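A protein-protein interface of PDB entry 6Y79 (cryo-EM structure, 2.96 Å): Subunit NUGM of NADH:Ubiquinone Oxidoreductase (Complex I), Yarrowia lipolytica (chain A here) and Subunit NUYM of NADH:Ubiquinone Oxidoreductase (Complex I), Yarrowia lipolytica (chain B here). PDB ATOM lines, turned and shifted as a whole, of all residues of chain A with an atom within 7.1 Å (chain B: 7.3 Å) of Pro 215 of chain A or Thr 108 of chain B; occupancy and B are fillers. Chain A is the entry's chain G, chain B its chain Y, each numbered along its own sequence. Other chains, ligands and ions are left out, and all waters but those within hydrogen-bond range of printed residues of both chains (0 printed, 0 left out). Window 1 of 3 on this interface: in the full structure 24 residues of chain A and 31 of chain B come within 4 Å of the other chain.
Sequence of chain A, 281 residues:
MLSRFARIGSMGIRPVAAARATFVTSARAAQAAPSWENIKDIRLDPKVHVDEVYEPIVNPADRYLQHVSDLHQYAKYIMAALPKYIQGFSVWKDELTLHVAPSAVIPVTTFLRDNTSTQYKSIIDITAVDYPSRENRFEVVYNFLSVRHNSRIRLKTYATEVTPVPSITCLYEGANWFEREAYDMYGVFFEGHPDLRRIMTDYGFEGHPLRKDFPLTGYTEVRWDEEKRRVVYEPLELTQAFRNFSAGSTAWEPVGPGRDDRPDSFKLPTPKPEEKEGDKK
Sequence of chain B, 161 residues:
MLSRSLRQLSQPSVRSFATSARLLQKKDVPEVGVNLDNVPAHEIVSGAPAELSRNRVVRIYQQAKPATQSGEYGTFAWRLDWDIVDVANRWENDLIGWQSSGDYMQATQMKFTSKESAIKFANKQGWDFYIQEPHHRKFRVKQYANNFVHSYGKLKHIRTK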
ATOM      1  N   PRO A 209       7.937 -16.913  23.767  1.00  0.00           N
ATOM      2  CA  PRO A 209       7.084 -15.966  23.048  1.00  0.00           C
ATOM      3  C   PRO A 209       7.270 -14.504  23.388  1.00  0.00           C
ATOM      4  O   PRO A 209       7.236 -13.652  22.499  1.00  0.00           O
ATOM      5  CB  PRO A 209       5.686 -16.425  23.440  1.00  0.00           C
ATOM      6  CG  PRO A 209       5.845 -17.837  23.738  1.00  0.00           C
ATOM      7  CD  PRO A 209       7.125 -17.913  24.469  1.00  0.00           C
ATOM      8  N   ARG A 211       9.278 -12.056  23.754  1.00  0.00           N
ATOM      9  CA  ARG A 211      10.678 -11.849  23.456  1.00  0.00           C
ATOM     10  C   ARG A 211      10.725 -11.138  22.124  1.00  0.00           C
ATOM     11  O   ARG A 211      10.014 -11.525  21.197  1.00  0.00           O
ATOM     12  CB  ARG A 211      11.411 -13.187  23.414  1.00  0.00           C
ATOM     13  CG  ARG A 211      12.882 -13.097  23.503  1.00  0.00           C
ATOM     14  CD  ARG A 211      13.510 -14.453  23.348  1.00  0.00           C
ATOM     15  NE  ARG A 211      13.856 -15.039  24.631  1.00  0.00           N
ATOM     16  CZ  ARG A 211      14.618 -16.116  24.771  1.00  0.00           C
ATOM     17  NH1 ARG A 211      15.110 -16.719  23.705  1.00  0.00           N
ATOM     18  NH2 ARG A 211      14.892 -16.587  25.975  1.00  0.00           N
ATOM     19  N   LYS A 212      11.549 -10.099  22.039  1.00  0.00           N
ATOM     20  CA  LYS A 212      11.454  -9.155  20.936  1.00  0.00           C
ATOM     21  C   LYS A 212      11.866  -9.743  19.591  1.00  0.00           C
ATOM     22  O   LYS A 212      11.503  -9.180  18.557  1.00  0.00           O
ATOM     23  CB  LYS A 212      12.288  -7.925  21.258  1.00  0.00           C
ATOM     24  CG  LYS A 212      11.886  -7.260  22.551  1.00  0.00           C
ATOM     25  CD  LYS A 212      10.497  -6.706  22.453  1.00  0.00           C
ATOM     26  CE  LYS A 212      10.106  -5.964  23.699  1.00  0.00           C
ATOM     27  NZ  LYS A 212       8.774  -5.322  23.525  1.00  0.00           N
ATOM     28  N   ASP A 213      12.594 -10.857  19.569  1.00  0.00           N
ATOM     29  CA  ASP A 213      12.903 -11.493  18.298  1.00  0.00           C
ATOM     30  C   ASP A 213      11.825 -12.461  17.839  1.00  0.00           C
ATOM     31  O   ASP A 213      11.784 -12.804  16.655  1.00  0.00           O
ATOM     32  CB  ASP A 213      14.270 -12.196  18.364  1.00  0.00           C
ATOM     33  CG  ASP A 213      14.339 -13.288  19.415  1.00  0.00           C
ATOM     34  OD1 ASP A 213      13.419 -13.410  20.242  1.00  0.00           O
ATOM     35  OD2 ASP A 213      15.331 -14.043  19.412  1.00  0.00           O
ATOM     36  N   PHE A 214      10.965 -12.899  18.744  1.00  0.00           N
ATOM     37  CA  PHE A 214       9.847 -13.765  18.405  1.00  0.00           C
ATOM     38  C   PHE A 214       8.757 -12.932  17.739  1.00  0.00           C
ATOM     39  O   PHE A 214       8.354 -11.907  18.290  1.00  0.00           O
ATOM     40  CB  PHE A 214       9.334 -14.441  19.677  1.00  0.00           C
ATOM     41  CG  PHE A 214       8.301 -15.501  19.448  1.00  0.00           C
ATOM     42  CD1 PHE A 214       8.655 -16.792  19.149  1.00  0.00           C
ATOM     43  CD2 PHE A 214       6.966 -15.205  19.591  1.00  0.00           C
ATOM     44  CE1 PHE A 214       7.688 -17.749  18.957  1.00  0.00           C
ATOM     45  CE2 PHE A 214       6.004 -16.149  19.385  1.00  0.00           C
ATOM     46  CZ  PHE A 214       6.367 -17.421  19.071  1.00  0.00           C
ATOM     47  N   PRO A 215       8.283 -13.312  16.553  1.00  0.00           N
ATOM     48  CA  PRO A 215       7.249 -12.521  15.879  1.00  0.00           C
ATOM     49  C   PRO A 215       5.896 -12.703  16.550  1.00  0.00           C
ATOM     50  O   PRO A 215       5.702 -13.586  17.373  1.00  0.00           O
ATOM     51  CB  PRO A 215       7.252 -13.085  14.462  1.00  0.00           C
ATOM     52  CG  PRO A 215       7.682 -14.468  14.643  1.00  0.00           C
ATOM     53  CD  PRO A 215       8.693 -14.461  15.737  1.00  0.00           C
ATOM     54  N   LEU A 216       4.942 -11.852  16.176  1.00  0.00           N
ATOM     55  CA  LEU A 216       3.645 -11.855  16.847  1.00  0.00           C
ATOM     56  C   LEU A 216       2.868 -13.133  16.569  1.00  0.00           C
ATOM     57  O   LEU A 216       2.430 -13.822  17.493  1.00  0.00           O
ATOM     58  CB  LEU A 216       2.828 -10.647  16.412  1.00  0.00           C
ATOM     59  CG  LEU A 216       1.456 -10.597  17.069  1.00  0.00           C
ATOM     60  CD1 LEU A 216       1.544 -10.533  18.585  1.00  0.00           C
ATOM     61  CD2 LEU A 216       0.639  -9.465  16.527  1.00  0.00           C
ATOM     62  N   THR A 217       2.693 -13.466  15.298  1.00  0.00           N
ATOM     63  CA  THR A 217       1.857 -14.589  14.929  1.00  0.00           C
ATOM     64  C   THR A 217       2.613 -15.909  15.066  1.00  0.00           C
ATOM     65  O   THR A 217       1.993 -16.973  15.104  1.00  0.00           O
ATOM     66  CB  THR A 217       1.344 -14.312  13.519  1.00  0.00           C
ATOM     67  OG1 THR A 217       0.903 -12.956  13.467  1.00  0.00           O
ATOM     68  CG2 THR A 217       0.169 -15.133  13.177  1.00  0.00           C
ATOM     69  N   GLY A 218       3.932 -15.860  15.183  1.00  0.00           N
ATOM     70  CA  GLY A 218       4.727 -17.031  15.480  1.00  0.00           C
ATOM     71  C   GLY A 218       5.372 -17.638  14.255  1.00  0.00           C
ATOM     72  O   GLY A 218       5.594 -16.987  13.234  1.00  0.00           O
ATOM     73  N   TYR A 219       5.691 -18.923  14.376  1.00  0.00           N
ATOM     74  CA  TYR A 219       6.343 -19.681  13.318  1.00  0.00           C
ATOM     75  C   TYR A 219       5.448 -20.732  12.692  1.00  0.00           C
ATOM     76  O   TYR A 219       5.560 -20.990  11.496  1.00  0.00           O
ATOM     77  CB  TYR A 219       7.604 -20.363  13.855  1.00  0.00           C
ATOM     78  CG  TYR A 219       8.632 -19.406  14.395  1.00  0.00           C
ATOM     79  CD1 TYR A 219       9.442 -18.692  13.544  1.00  0.00           C
ATOM     80  CD2 TYR A 219       8.796 -19.221  15.752  1.00  0.00           C
ATOM     81  CE1 TYR A 219      10.382 -17.810  14.027  1.00  0.00           C
ATOM     82  CE2 TYR A 219       9.738 -18.345  16.236  1.00  0.00           C
ATOM     83  CZ  TYR A 219      10.520 -17.638  15.368  1.00  0.00           C
ATOM     84  OH  TYR A 219      11.460 -16.762  15.844  1.00  0.00           O
ATOM     85  N   LEU A 236       3.893 -21.126   9.042  1.00  0.00           N
ATOM     86  CA  LEU A 236       2.759 -20.231   9.180  1.00  0.00           C
ATOM     87  C   LEU A 236       2.466 -19.490   7.888  1.00  0.00           C
ATOM     88  O   LEU A 236       3.372 -19.132   7.133  1.00  0.00           O
ATOM     89  CB  LEU A 236       3.032 -19.242  10.297  1.00  0.00           C
ATOM     90  CG  LEU A 236       2.030 -18.158  10.653  1.00  0.00           C
ATOM     91  CD1 LEU A 236       0.710 -18.735  11.084  1.00  0.00           C
ATOM     92  CD2 LEU A 236       2.654 -17.417  11.761  1.00  0.00           C
ATOM     93  N   PHE A 242      -0.556  -9.362   8.997  1.00  0.00           N
ATOM     94  CA  PHE A 242      -0.636  -8.439  10.118  1.00  0.00           C
ATOM     95  C   PHE A 242      -0.143  -7.069   9.693  1.00  0.00           C
ATOM     96  O   PHE A 242       0.907  -6.943   9.062  1.00  0.00           O
ATOM     97  CB  PHE A 242       0.181  -8.957  11.293  1.00  0.00           C
ATOM     98  CG  PHE A 242       0.166  -8.055  12.478  1.00  0.00           C
ATOM     99  CD1 PHE A 242      -0.976  -7.904  13.233  1.00  0.00           C
ATOM    100  CD2 PHE A 242       1.294  -7.358  12.843  1.00  0.00           C
ATOM    101  CE1 PHE A 242      -0.989  -7.078  14.326  1.00  0.00           C
ATOM    102  CE2 PHE A 242       1.281  -6.528  13.933  1.00  0.00           C
ATOM    103  CZ  PHE A 242       0.134  -6.385  14.669  1.00  0.00           C
ATOM    104  N   ASN A 244       0.895  -3.626  11.308  1.00  0.00           N
ATOM    105  CA  ASN A 244       1.093  -2.784  12.470  1.00  0.00           C
ATOM    106  C   ASN A 244       1.114  -1.321  12.062  1.00  0.00           C
ATOM    107  O   ASN A 244       1.654  -0.940  11.022  1.00  0.00           O
ATOM    108  CB  ASN A 244       2.348  -3.158  13.267  1.00  0.00           C
ATOM    109  CG  ASN A 244       3.615  -3.092  12.477  1.00  0.00           C
ATOM    110  OD1 ASN A 244       3.615  -2.959  11.257  1.00  0.00           O
ATOM    111  ND2 ASN A 244       4.731  -3.193  13.184  1.00  0.00           N
ATOM    112  N   LEU B  52      15.748 -19.201   9.294  1.00  0.00           N
ATOM    113  CA  LEU B  52      15.789 -17.764   9.522  1.00  0.00           C
ATOM    114  C   LEU B  52      17.218 -17.264   9.622  1.00  0.00           C
ATOM    115  O   LEU B  52      17.542 -16.170   9.147  1.00  0.00           O
ATOM    116  CB  LEU B  52      15.011 -17.436  10.797  1.00  0.00           C
ATOM    117  CG  LEU B  52      14.834 -15.984  11.213  1.00  0.00           C
ATOM    118  CD1 LEU B  52      13.973 -15.258  10.200  1.00  0.00           C
ATOM    119  CD2 LEU B  52      14.224 -15.936  12.594  1.00  0.00           C
ATOM    120  N   LEU B  80      15.980  -2.671  13.498  1.00  0.00           N
ATOM    121  CA  LEU B  80      16.376  -3.942  12.915  1.00  0.00           C
ATOM    122  C   LEU B  80      15.188  -4.512  12.158  1.00  0.00           C
ATOM    123  O   LEU B  80      14.095  -4.637  12.722  1.00  0.00           O
ATOM    124  CB  LEU B  80      16.840  -4.914  13.996  1.00  0.00           C
ATOM    125  CG  LEU B  80      17.324  -6.293  13.567  1.00  0.00           C
ATOM    126  CD1 LEU B  80      18.629  -6.163  12.878  1.00  0.00           C
ATOM    127  CD2 LEU B  80      17.487  -7.165  14.770  1.00  0.00           C
ATOM    128  N   ASP B  81      15.408  -4.865  10.893  1.00  0.00           N
ATOM    129  CA  ASP B  81      14.321  -5.071   9.948  1.00  0.00           C
ATOM    130  C   ASP B  81      14.748  -6.097   8.912  1.00  0.00           C
ATOM    131  O   ASP B  81      15.852  -6.020   8.388  1.00  0.00           O
ATOM    132  CB  ASP B  81      13.985  -3.739   9.279  1.00  0.00           C
ATOM    133  CG  ASP B  81      12.716  -3.767   8.470  1.00  0.00           C
ATOM    134  OD1 ASP B  81      12.017  -4.799   8.413  1.00  0.00           O
ATOM    135  OD2 ASP B  81      12.419  -2.719   7.860  1.00  0.00           O
ATOM    136  N   TRP B  82      13.859  -7.017   8.575  1.00  0.00           N
ATOM    137  CA  TRP B  82      14.203  -8.131   7.709  1.00  0.00           C
ATOM    138  C   TRP B  82      13.946  -7.777   6.256  1.00  0.00           C
ATOM    139  O   TRP B  82      12.943  -7.142   5.927  1.00  0.00           O
ATOM    140  CB  TRP B  82      13.420  -9.382   8.103  1.00  0.00           C
ATOM    141  CG  TRP B  82      13.941  -9.969   9.359  1.00  0.00           C
ATOM    142  CD1 TRP B  82      14.805 -11.012   9.478  1.00  0.00           C
ATOM    143  CD2 TRP B  82      13.675  -9.514  10.687  1.00  0.00           C
ATOM    144  NE1 TRP B  82      15.082 -11.246  10.802  1.00  0.00           N
ATOM    145  CE2 TRP B  82      14.398 -10.337  11.564  1.00  0.00           C
ATOM    146  CE3 TRP B  82      12.884  -8.497  11.222  1.00  0.00           C
ATOM    147  CZ2 TRP B  82      14.361 -10.167  12.937  1.00  0.00           C
ATOM    148  CZ3 TRP B  82      12.851  -8.331  12.579  1.00  0.00           C
ATOM    149  CH2 TRP B  82      13.575  -9.164  13.424  1.00  0.00           C
ATOM    150  N   TYR B 104       6.718 -14.158   7.780  1.00  0.00           N
ATOM    151  CA  TYR B 104       6.216 -13.873   9.112  1.00  0.00           C
ATOM    152  C   TYR B 104       7.036 -12.844   9.876  1.00  0.00           C
ATOM    153  O   TYR B 104       6.569 -12.352  10.906  1.00  0.00           O
ATOM    154  CB  TYR B 104       6.125 -15.170   9.928  1.00  0.00           C
ATOM    155  CG  TYR B 104       7.417 -15.932  10.023  1.00  0.00           C
ATOM    156  CD1 TYR B 104       8.327 -15.646  11.018  1.00  0.00           C
ATOM    157  CD2 TYR B 104       7.724 -16.951   9.130  1.00  0.00           C
ATOM    158  CE1 TYR B 104       9.508 -16.298  11.106  1.00  0.00           C
ATOM    159  CE2 TYR B 104       8.918 -17.635   9.228  1.00  0.00           C
ATOM    160  CZ  TYR B 104       9.800 -17.299  10.232  1.00  0.00           C
ATOM    161  OH  TYR B 104      10.995 -17.953  10.369  1.00  0.00           O
ATOM    162  N   MET B 105       8.243 -12.523   9.421  1.00  0.00           N
ATOM    163  CA  MET B 105       9.033 -11.461  10.022  1.00  0.00           C
ATOM    164  C   MET B 105       8.785 -10.112   9.365  1.00  0.00           C
ATOM    165  O   MET B 105       9.602  -9.200   9.531  1.00  0.00           O
ATOM    166  CB  MET B 105      10.524 -11.798   9.960  1.00  0.00           C
ATOM    167  CG  MET B 105      10.955 -13.020  10.745  1.00  0.00           C
ATOM    168  SD  MET B 105      10.305 -13.108  12.417  1.00  0.00           S
ATOM    169  CE  MET B 105      11.525 -12.245  13.359  1.00  0.00           C
ATOM    170  N   GLN B 106       7.682  -9.963   8.626  1.00  0.00           N
ATOM    171  CA  GLN B 106       7.461  -8.732   7.874  1.00  0.00           C
ATOM    172  C   GLN B 106       7.022  -7.587   8.772  1.00  0.00           C
ATOM    173  O   GLN B 106       7.246  -6.421   8.439  1.00  0.00           O
ATOM    174  CB  GLN B 106       6.435  -8.964   6.765  1.00  0.00           C
ATOM    175  CG  GLN B 106       5.078  -9.468   7.223  1.00  0.00           C
ATOM    176  CD  GLN B 106       4.060  -8.356   7.425  1.00  0.00           C
ATOM    177  OE1 GLN B 106       4.170  -7.276   6.847  1.00  0.00           O
ATOM    178  NE2 GLN B 106       3.067  -8.620   8.254  1.00  0.00           N
ATOM    179  N   ALA B 107       6.403  -7.890   9.904  1.00  0.00           N
ATOM    180  CA  ALA B 107       5.928  -6.853  10.802  1.00  0.00           C
ATOM    181  C   ALA B 107       6.811  -6.677  12.023  1.00  0.00           C
ATOM    182  O   ALA B 107       6.656  -5.685  12.740  1.00  0.00           O
ATOM    183  CB  ALA B 107       4.499  -7.158  11.248  1.00  0.00           C
ATOM    184  N   THR B 108       7.715  -7.615  12.283  1.00  0.00           N
ATOM    185  CA  THR B 108       8.639  -7.475  13.394  1.00  0.00           C
ATOM    186  C   THR B 108       9.699  -6.438  13.056  1.00  0.00           C
ATOM    187  O   THR B 108      10.236  -6.409  11.947  1.00  0.00           O
ATOM    188  CB  THR B 108       9.285  -8.820  13.719  1.00  0.00           C
ATOM    189  OG1 THR B 108       8.272  -9.828  13.763  1.00  0.00           O
ATOM    190  CG2 THR B 108       9.987  -8.778  15.070  1.00  0.00           C
ATOM    191  N   GLN B 109       9.982  -5.566  14.018  1.00  0.00           N
ATOM    192  CA  GLN B 109      10.992  -4.532  13.855  1.00  0.00           C
ATOM    193  C   GLN B 109      11.512  -4.178  15.233  1.00  0.00           C
ATOM    194  O   GLN B 109      10.721  -3.965  16.152  1.00  0.00           O
ATOM    195  CB  GLN B 109      10.414  -3.303  13.167  1.00  0.00           C
ATOM    196  CG  GLN B 109      11.404  -2.191  12.955  1.00  0.00           C
ATOM    197  CD  GLN B 109      10.851  -1.114  12.062  1.00  0.00           C
ATOM    198  OE1 GLN B 109       9.657  -1.091  11.773  1.00  0.00           O
ATOM    199  NE2 GLN B 109      11.714  -0.225  11.604  1.00  0.00           N
ATOM    200  N   MET B 110      12.828  -4.119  15.380  1.00  0.00           N
ATOM    201  CA  MET B 110      13.422  -3.898  16.685  1.00  0.00           C
ATOM    202  C   MET B 110      13.989  -2.498  16.810  1.00  0.00           C
ATOM    203  O   MET B 110      14.420  -1.899  15.827  1.00  0.00           O
ATOM    204  CB  MET B 110      14.535  -4.883  16.958  1.00  0.00           C
ATOM    205  CG  MET B 110      14.088  -6.280  17.016  1.00  0.00           C
ATOM    206  SD  MET B 110      15.281  -7.215  17.947  1.00  0.00           S
ATOM    207  CE  MET B 110      15.016  -8.753  17.134  1.00  0.00           C
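The backbone carbonyl oxygen of Ala 107 of chain B is in hydrogen-bond range of the side-chain amide nitrogen of Asn 244 of chain A, at 3.2 Å.
NE2 of Gln 106 of chain B sits at hydrogen-bond distance from O of Phe 242 of chain A (2.9 Å).
O of Met 110 of chain B is in hydrogen-bond range of N of Leu 80 of chain B, at 2.9 Å.
The backbone carbonyl oxygen (O) of Tyr 219 of chain A is in hydrogen-bond range of the backbone NH (N) of Leu 236 of chain A (3.0 Å).
CG2 of Thr 108 of chain B touches O of Lys 212 of chain A (3.8 Å).
Met 110 of chain B touches Lys 212 of chain A (CE to O, 3.8 Å).
O of Asp 213 of chain A touches CE of Met 105 of chain B (3.4 Å).
CE of Met 110 of chain B touches CA of Asp 213 of chain A (3.7 Å).
Pro 215 of chain A touches Tyr 104 of chain B.
CB of Pro 215 of chain A touches SD of Met 105 of chain B, at 3.7 Å.
Thr 108 of chain B touches Pro 215 of chain A (OG1 to CB, 3.5 Å).
O of Gly 218 of chain A touches CD1 of Tyr 104 of chain B, at 3.8 Å.
Tyr 219 of chain A touches Tyr 104 of chain B (CE1 to CE1, 3.4 Å).
Phe 242 of chain A touches Ala 107 of chain B (CD2 to CB, 3.6 Å).
Pro 215 of chain A touches just these residues of chain B: Tyr 104 (3.7 Å), Met 105 (3.7 Å) and Thr 108 (3.5 Å).
Leu 236 of chain A touches none of the printed residues of chain B.
Of the printed residues of chain B, Phe 242 of chain A touches Gln 106 and Ala 107.
Of the printed residues of chain A, Tyr 104 of chain B touches Pro 215 (3.7 Å), Gly 218 (3.8 Å) and Tyr 219 (3.4 Å).
Printed residues of chain A within 4 Å of Met 105 of chain B: Asp 213 (3.4 Å) and Pro 215 (3.7 Å).
Of chain A, only Lys 212 (3.8 Å) and Pro 215 (3.5 Å) come within 4 Å of Thr 108 of chain B.
Of the printed residues of chain A, Met 110 of chain B touches Lys 212 (3.8 Å) and Asp 213 (3.7 Å).
The nearest residue of chain B that does not touch Pro 215 of chain A is Leu 52 of chain B (6.5 Å).
The nearest residue of chain A that does not touch Thr 108 of chain B is Leu 216 of chain A (4.6 Å).
Printed residues of chain B that touch a printed residue of chain A: Tyr 104, Met 105, Gln 106, Ala 107, Thr 108 and Met 110.
Hydrophobic or aromatic side chains of chain B that line the printed part of chain A: Tyr 104, Met 105, Ala 107 and Met 110.
Hydrophobic or aromatic side chains of chain A within 4 Å of the printed part of chain B: Pro 215, Tyr 219 and Phe 242.
Among the printed residues, no Asp or Glu carboxylate lies within 4 Å of a Lys or Arg side-chain nitrogen of the other chain.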
